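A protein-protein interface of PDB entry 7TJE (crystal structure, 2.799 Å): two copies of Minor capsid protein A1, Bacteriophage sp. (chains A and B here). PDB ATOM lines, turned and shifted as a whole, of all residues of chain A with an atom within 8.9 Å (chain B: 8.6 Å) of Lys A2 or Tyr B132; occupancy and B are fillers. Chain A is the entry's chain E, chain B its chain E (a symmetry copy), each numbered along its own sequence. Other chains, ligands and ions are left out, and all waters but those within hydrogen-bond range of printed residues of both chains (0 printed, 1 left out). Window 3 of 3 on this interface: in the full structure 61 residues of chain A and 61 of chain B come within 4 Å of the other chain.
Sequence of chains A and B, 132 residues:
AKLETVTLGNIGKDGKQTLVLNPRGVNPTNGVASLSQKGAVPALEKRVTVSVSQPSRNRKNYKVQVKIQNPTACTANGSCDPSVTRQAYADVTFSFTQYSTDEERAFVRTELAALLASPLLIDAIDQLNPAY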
ATOM      1  N   ALA A   1      10.334  -0.215  -0.573  1.00  0.00           N
ATOM      2  CA  ALA A   1      10.370  -1.659  -0.423  1.00  0.00           C
ATOM      3  C   ALA A   1      11.813  -2.163  -0.519  1.00  0.00           C
ATOM      4  O   ALA A   1      12.665  -1.518  -1.140  1.00  0.00           O
ATOM      5  CB  ALA A   1       9.484  -2.333  -1.465  1.00  0.00           C
ATOM      6  N   LYS A   2      12.076  -3.296   0.140  1.00  0.00           N
ATOM      7  CA  LYS A   2      13.399  -3.908   0.203  1.00  0.00           C
ATOM      8  C   LYS A   2      14.043  -3.948  -1.171  1.00  0.00           C
ATOM      9  O   LYS A   2      13.550  -4.637  -2.068  1.00  0.00           O
ATOM     10  CB  LYS A   2      13.299  -5.328   0.769  1.00  0.00           C
ATOM     11  CG  LYS A   2      14.621  -6.070   0.896  1.00  0.00           C
ATOM     12  CD  LYS A   2      15.559  -5.390   1.877  1.00  0.00           C
ATOM     13  CE  LYS A   2      16.790  -6.247   2.130  1.00  0.00           C
ATOM     14  NZ  LYS A   2      17.973  -5.387   2.391  1.00  0.00           N
ATOM     15  N   LEU A   3      15.118  -3.188  -1.361  1.00  0.00           N
ATOM     16  CA  LEU A   3      15.921  -3.362  -2.565  1.00  0.00           C
ATOM     17  C   LEU A   3      16.455  -4.784  -2.598  1.00  0.00           C
ATOM     18  O   LEU A   3      17.550  -5.069  -2.109  1.00  0.00           O
ATOM     19  CB  LEU A   3      17.057  -2.351  -2.617  1.00  0.00           C
ATOM     20  CG  LEU A   3      17.469  -1.880  -4.004  1.00  0.00           C
ATOM     21  CD1 LEU A   3      16.294  -1.894  -4.964  1.00  0.00           C
ATOM     22  CD2 LEU A   3      18.031  -0.491  -3.846  1.00  0.00           C
ATOM     23  N   GLU A   4      15.661  -5.686  -3.141  1.00  0.00           N
ATOM     24  CA  GLU A   4      15.975  -7.098  -3.209  1.00  0.00           C
ATOM     25  C   GLU A   4      16.014  -7.518  -4.670  1.00  0.00           C
ATOM     26  O   GLU A   4      15.641  -6.767  -5.576  1.00  0.00           O
ATOM     27  CB  GLU A   4      14.945  -7.942  -2.424  1.00  0.00           C
ATOM     28  CG  GLU A   4      13.480  -7.615  -2.766  1.00  0.00           C
ATOM     29  CD  GLU A   4      12.532  -8.806  -2.701  1.00  0.00           C
ATOM     30  OE1 GLU A   4      12.958  -9.937  -3.030  1.00  0.00           O
ATOM     31  OE2 GLU A   4      11.347  -8.600  -2.354  1.00  0.00           O
ATOM     32  N   THR A   5      16.479  -8.739  -4.886  1.00  0.00           N
ATOM     33  CA  THR A   5      16.484  -9.293  -6.228  1.00  0.00           C
ATOM     34  C   THR A   5      15.058  -9.402  -6.760  1.00  0.00           C
ATOM     35  O   THR A   5      14.294 -10.285  -6.353  1.00  0.00           O
ATOM     36  CB  THR A   5      17.197 -10.642  -6.237  1.00  0.00           C
ATOM     37  OG1 THR A   5      18.614 -10.415  -6.220  1.00  0.00           O
ATOM     38  CG2 THR A   5      16.865 -11.431  -7.484  1.00  0.00           C
ATOM     39  N   VAL A   6      14.683  -8.478  -7.656  1.00  0.00           N
ATOM     40  CA  VAL A   6      13.398  -8.554  -8.342  1.00  0.00           C
ATOM     41  C   VAL A   6      13.517  -9.534  -9.496  1.00  0.00           C
ATOM     42  O   VAL A   6      14.510  -9.550 -10.224  1.00  0.00           O
ATOM     43  CB  VAL A   6      12.955  -7.162  -8.827  1.00  0.00           C
ATOM     44  CG1 VAL A   6      12.706  -6.245  -7.643  1.00  0.00           C
ATOM     45  CG2 VAL A   6      14.018  -6.571  -9.686  1.00  0.00           C
ATOM     46  N   PRO A  23      20.026  -6.303  -6.622  1.00  0.00           N
ATOM     47  CA  PRO A  23      20.318  -4.961  -6.094  1.00  0.00           C
ATOM     48  C   PRO A  23      21.765  -4.589  -6.347  1.00  0.00           C
ATOM     49  O   PRO A  23      22.675  -5.385  -6.119  1.00  0.00           O
ATOM     50  CB  PRO A  23      20.027  -5.092  -4.595  1.00  0.00           C
ATOM     51  CG  PRO A  23      19.990  -6.598  -4.334  1.00  0.00           C
ATOM     52  CD  PRO A  23      19.522  -7.230  -5.599  1.00  0.00           C
ATOM     53  N   ARG A  24      21.979  -3.371  -6.826  1.00  0.00           N
ATOM     54  CA  ARG A  24      23.290  -2.994  -7.335  1.00  0.00           C
ATOM     55  C   ARG A  24      23.573  -1.545  -7.013  1.00  0.00           C
ATOM     56  O   ARG A  24      24.160  -0.810  -7.818  1.00  0.00           O
ATOM     57  CB  ARG A  24      23.401  -3.235  -8.846  1.00  0.00           C
ATOM     58  CG  ARG A  24      23.609  -4.688  -9.241  1.00  0.00           C
ATOM     59  CD  ARG A  24      25.061  -5.078  -9.130  1.00  0.00           C
ATOM     60  NE  ARG A  24      25.921  -3.966  -9.512  1.00  0.00           N
ATOM     61  CZ  ARG A  24      26.708  -3.970 -10.586  1.00  0.00           C
ATOM     62  NH1 ARG A  24      26.736  -5.023 -11.403  1.00  0.00           N
ATOM     63  NH2 ARG A  24      27.458  -2.911 -10.862  1.00  0.00           N
ATOM     64  N   GLY A  25      23.142  -1.110  -5.840  1.00  0.00           N
ATOM     65  CA  GLY A  25      23.467   0.225  -5.369  1.00  0.00           C
ATOM     66  C   GLY A  25      22.225   1.037  -5.079  1.00  0.00           C
ATOM     67  O   GLY A  25      21.114   0.698  -5.493  1.00  0.00           O
ATOM     68  N   VAL A  26      22.407   2.105  -4.315  1.00  0.00           N
ATOM     69  CA  VAL A  26      21.430   3.176  -4.185  1.00  0.00           C
ATOM     70  C   VAL A  26      22.254   4.440  -4.370  1.00  0.00           C
ATOM     71  O   VAL A  26      23.421   4.364  -4.762  1.00  0.00           O
ATOM     72  CB  VAL A  26      20.701   3.140  -2.825  1.00  0.00           C
ATOM     73  CG1 VAL A  26      19.396   3.909  -2.871  1.00  0.00           C
ATOM     74  CG2 VAL A  26      20.434   1.707  -2.386  1.00  0.00           C
ATOM     75  N   ASN A  27      21.654   5.597  -4.147  1.00  0.00           N
ATOM     76  CA  ASN A  27      22.401   6.768  -3.704  1.00  0.00           C
ATOM     77  C   ASN A  27      23.666   7.102  -4.499  1.00  0.00           C
ATOM     78  O   ASN A  27      24.665   7.485  -3.880  1.00  0.00           O
ATOM     79  CB  ASN A  27      22.778   6.541  -2.230  1.00  0.00           C
ATOM     80  CG  ASN A  27      22.882   7.826  -1.424  1.00  0.00           C
ATOM     81  OD1 ASN A  27      22.567   7.837  -0.231  1.00  0.00           O
ATOM     82  ND2 ASN A  27      23.348   8.894  -2.048  1.00  0.00           N
ATOM     83  N   GLY A  31      19.921   9.462  -5.349  1.00  0.00           N
ATOM     84  CA  GLY A  31      18.857   8.649  -4.809  1.00  0.00           C
ATOM     85  C   GLY A  31      18.299   7.581  -5.721  1.00  0.00           C
ATOM     86  O   GLY A  31      17.324   6.923  -5.336  1.00  0.00           O
ATOM     87  N   VAL A  32      18.868   7.363  -6.905  1.00  0.00           N
ATOM     88  CA  VAL A  32      18.287   6.376  -7.808  1.00  0.00           C
ATOM     89  C   VAL A  32      18.821   4.994  -7.428  1.00  0.00           C
ATOM     90  O   VAL A  32      20.018   4.716  -7.501  1.00  0.00           O
ATOM     91  CB  VAL A  32      18.521   6.728  -9.289  1.00  0.00           C
ATOM     92  CG1 VAL A  32      18.257   8.212  -9.512  1.00  0.00           C
ATOM     93  CG2 VAL A  32      19.893   6.341  -9.828  1.00  0.00           C
ATOM     94  N   ALA A  33      17.933   4.158  -6.917  1.00  0.00           N
ATOM     95  CA  ALA A  33      18.219   2.737  -6.789  1.00  0.00           C
ATOM     96  C   ALA A  33      18.545   2.128  -8.154  1.00  0.00           C
ATOM     97  O   ALA A  33      18.027   2.555  -9.189  1.00  0.00           O
ATOM     98  CB  ALA A  33      17.018   2.026  -6.171  1.00  0.00           C
ATOM     99  N   SER A  34      19.409   1.110  -8.153  1.00  0.00           N
ATOM    100  CA  SER A  34      19.815   0.464  -9.389  1.00  0.00           C
ATOM    101  C   SER A  34      19.703  -1.047  -9.249  1.00  0.00           C
ATOM    102  O   SER A  34      19.978  -1.619  -8.194  1.00  0.00           O
ATOM    103  CB  SER A  34      21.237   0.865  -9.789  1.00  0.00           C
ATOM    104  OG  SER A  34      21.436   2.265  -9.655  1.00  0.00           O
ATOM    105  N   LEU A  35      19.267  -1.688 -10.313  1.00  0.00           N
ATOM    106  CA  LEU A  35      19.283  -3.129 -10.403  1.00  0.00           C
ATOM    107  C   LEU A  35      19.990  -3.500 -11.699  1.00  0.00           C
ATOM    108  O   LEU A  35      20.208  -2.656 -12.575  1.00  0.00           O
ATOM    109  CB  LEU A  35      17.864  -3.701 -10.357  1.00  0.00           C
ATOM    110  CG  LEU A  35      16.961  -3.073  -9.288  1.00  0.00           C
ATOM    111  CD1 LEU A  35      15.511  -3.216  -9.695  1.00  0.00           C
ATOM    112  CD2 LEU A  35      17.192  -3.737  -7.952  1.00  0.00           C
ATOM    113  N   VAL A  50      15.155   3.169 -10.332  1.00  0.00           N
ATOM    114  CA  VAL A  50      13.922   3.694  -9.773  1.00  0.00           C
ATOM    115  C   VAL A  50      14.273   4.865  -8.874  1.00  0.00           C
ATOM    116  O   VAL A  50      15.222   4.792  -8.087  1.00  0.00           O
ATOM    117  CB  VAL A  50      13.148   2.627  -8.986  1.00  0.00           C
ATOM    118  CG1 VAL A  50      11.778   3.165  -8.645  1.00  0.00           C
ATOM    119  CG2 VAL A  50      13.042   1.328  -9.777  1.00  0.00           C
ATOM    120  N   PRO B 119       7.005  -5.639  -6.316  1.00  0.00           N
ATOM    121  CA  PRO B 119       6.951  -4.949  -5.015  1.00  0.00           C
ATOM    122  C   PRO B 119       7.736  -3.645  -4.990  1.00  0.00           C
ATOM    123  O   PRO B 119       7.243  -2.639  -4.458  1.00  0.00           O
ATOM    124  CB  PRO B 119       7.530  -5.993  -4.046  1.00  0.00           C
ATOM    125  CG  PRO B 119       7.303  -7.291  -4.711  1.00  0.00           C
ATOM    126  CD  PRO B 119       7.426  -7.044  -6.183  1.00  0.00           C
ATOM    127  N   LEU B 120       8.935  -3.626  -5.572  1.00  0.00           N
ATOM    128  CA  LEU B 120       9.708  -2.388  -5.609  1.00  0.00           C
ATOM    129  C   LEU B 120       8.916  -1.258  -6.264  1.00  0.00           C
ATOM    130  O   LEU B 120       8.907  -0.129  -5.756  1.00  0.00           O
ATOM    131  CB  LEU B 120      11.033  -2.608  -6.340  1.00  0.00           C
ATOM    132  CG  LEU B 120      11.983  -1.404  -6.403  1.00  0.00           C
ATOM    133  CD1 LEU B 120      12.636  -1.173  -5.048  1.00  0.00           C
ATOM    134  CD2 LEU B 120      13.047  -1.551  -7.501  1.00  0.00           C
ATOM    135  N   LEU B 121       8.241  -1.534  -7.387  1.00  0.00           N
ATOM    136  CA  LEU B 121       7.516  -0.457  -8.059  1.00  0.00           C
ATOM    137  C   LEU B 121       6.168  -0.173  -7.414  1.00  0.00           C
ATOM    138  O   LEU B 121       5.739   0.988  -7.385  1.00  0.00           O
ATOM    139  CB  LEU B 121       7.314  -0.764  -9.543  1.00  0.00           C
ATOM    140  CG  LEU B 121       8.439  -0.432 -10.529  1.00  0.00           C
ATOM    141  CD1 LEU B 121       8.781   1.039 -10.393  1.00  0.00           C
ATOM    142  CD2 LEU B 121       9.678  -1.316 -10.348  1.00  0.00           C
ATOM    143  N   ASP B 123       5.654  -0.209  -4.264  1.00  0.00           N
ATOM    144  CA  ASP B 123       5.922   0.691  -3.149  1.00  0.00           C
ATOM    145  C   ASP B 123       6.285   2.094  -3.626  1.00  0.00           C
ATOM    146  O   ASP B 123       5.871   3.088  -3.018  1.00  0.00           O
ATOM    147  CB  ASP B 123       7.023   0.117  -2.263  1.00  0.00           C
ATOM    148  CG  ASP B 123       6.847   0.505  -0.802  1.00  0.00           C
ATOM    149  OD1 ASP B 123       5.723   0.357  -0.258  1.00  0.00           O
ATOM    150  OD2 ASP B 123       7.838   0.966  -0.202  1.00  0.00           O
ATOM    151  N   ASN B 129       7.290   5.508  -1.754  1.00  0.00           N
ATOM    152  CA  ASN B 129       8.439   5.162  -0.923  1.00  0.00           C
ATOM    153  C   ASN B 129       9.658   4.953  -1.790  1.00  0.00           C
ATOM    154  O   ASN B 129       9.609   4.102  -2.689  1.00  0.00           O
ATOM    155  CB  ASN B 129       8.173   3.882  -0.141  1.00  0.00           C
ATOM    156  CG  ASN B 129       7.599   4.138   1.216  1.00  0.00           C
ATOM    157  OD1 ASN B 129       7.938   5.128   1.869  1.00  0.00           O
ATOM    158  ND2 ASN B 129       6.734   3.233   1.671  1.00  0.00           N
ATOM    159  N   PRO B 130      10.782   5.645  -1.554  1.00  0.00           N
ATOM    160  CA  PRO B 130      12.003   5.301  -2.296  1.00  0.00           C
ATOM    161  C   PRO B 130      12.473   3.891  -1.973  1.00  0.00           C
ATOM    162  O   PRO B 130      11.746   3.087  -1.376  1.00  0.00           O
ATOM    163  CB  PRO B 130      13.013   6.366  -1.843  1.00  0.00           C
ATOM    164  CG  PRO B 130      12.161   7.513  -1.356  1.00  0.00           C
ATOM    165  CD  PRO B 130      10.976   6.835  -0.706  1.00  0.00           C
ATOM    166  N   ALA B 131      13.699   3.576  -2.362  1.00  0.00           N
ATOM    167  CA  ALA B 131      14.236   2.237  -2.189  1.00  0.00           C
ATOM    168  C   ALA B 131      15.428   2.261  -1.241  1.00  0.00           C
ATOM    169  O   ALA B 131      16.211   3.225  -1.220  1.00  0.00           O
ATOM    170  CB  ALA B 131      14.633   1.628  -3.531  1.00  0.00           C
ATOM    171  N   TYR B 132      15.541   1.186  -0.463  1.00  0.00           N
ATOM    172  CA  TYR B 132      16.600   1.000   0.521  1.00  0.00           C
ATOM    173  C   TYR B 132      17.233  -0.377   0.370  1.00  0.00           C
ATOM    174  O   TYR B 132      18.456  -0.515   0.418  1.00  0.00           O
ATOM    175  CB  TYR B 132      16.046   1.161   1.933  1.00  0.00           C
ATOM    176  CG  TYR B 132      14.958   0.169   2.285  1.00  0.00           C
ATOM    177  CD1 TYR B 132      13.685   0.294   1.761  1.00  0.00           C
ATOM    178  CD2 TYR B 132      15.204  -0.889   3.155  1.00  0.00           C
ATOM    179  CE1 TYR B 132      12.693  -0.601   2.089  1.00  0.00           C
ATOM    180  CE2 TYR B 132      14.207  -1.800   3.489  1.00  0.00           C
ATOM    181  CZ  TYR B 132      12.953  -1.659   2.958  1.00  0.00           C
ATOM    182  OH  TYR B 132      11.971  -2.571   3.297  1.00  0.00           O
ATOM    183  OXT TYR B 132      16.524  -1.372   0.196  1.00  0.00           O
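N of Ala A1 lies within hydrogen-bond range of OD2 of Asp B123, at 2.8 Å. The backbone NH (N) of Lys A2 lies within hydrogen-bond range of the side-chain hydroxyl (OH) of Tyr B132 (3.2 Å). OXT of Tyr B132 is in hydrogen-bond range of N of Leu A3, 2.8 Å away.
The backbone NH (N) of Ala A33 sits at hydrogen-bond distance from the backbone carbonyl oxygen (O) of Val A50, 3.0 Å away. O of Asp B123 sits at hydrogen-bond distance from N of Asn B129 (3.1 Å).
Among the printed residues, pairs that only touch across the chains: Ala A1 with Tyr B132 (3.2 Å), Ala A33 with Ala B131 (3.6 Å), Val A26 with Ala B131 (3.7 Å), Val A50 with Leu B120 (3.7 Å), Ala A1 with Pro B130 (3.7 Å), Leu A35 with Leu B120 (3.7 Å), Leu A3 with Leu B120 (3.7 Å), Ala A1 with Pro B119 (3.8 Å) and Ala A1 with Leu B120 (3.9 Å).
Lys A2 touches one residue of chain B. Ala A1 touches five residues of chain B. Of the printed residues of chain A, Pro B130 touches Ala A1 (3.7 Å). Of the printed residues of chain B, Leu A35 touches Leu B120. Of the printed residues of chain A, Ala B131 touches Val A26 and Ala A33. Asn B129 touches none of the printed residues of chain A. Val A32 touches none of the printed residues of chain B. The nearest residue of chain B that does not touch Lys A2 is Leu B120 (4.7 Å). The nearest residue of chain A that does not touch Tyr B132 is Val A26 (4.1 Å).
Of the 17 printed residues of chain A, 7 touch a printed residue of chain B. Hydrophobic or aromatic side chains of chain A that line the printed part of chain B: Ala A1, Leu A3, Val A26, Ala A33, Leu A35 and Val A50. Hydrophobic or aromatic side chains of chain B within 4 Å of the printed part of chain A: Leu B120, Ala B131 and Tyr B132. Among the printed residues, 12 pairs touch across the chains. Among the printed residues, no Asp or Glu carboxylate lies within 4 Å of a Lys or Arg side-chain nitrogen of the other chain.
No position is printed for both chains. Of the 12 pairs that touch across the chains among the printed residues, none has its exchanged pair printed and touching as well.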
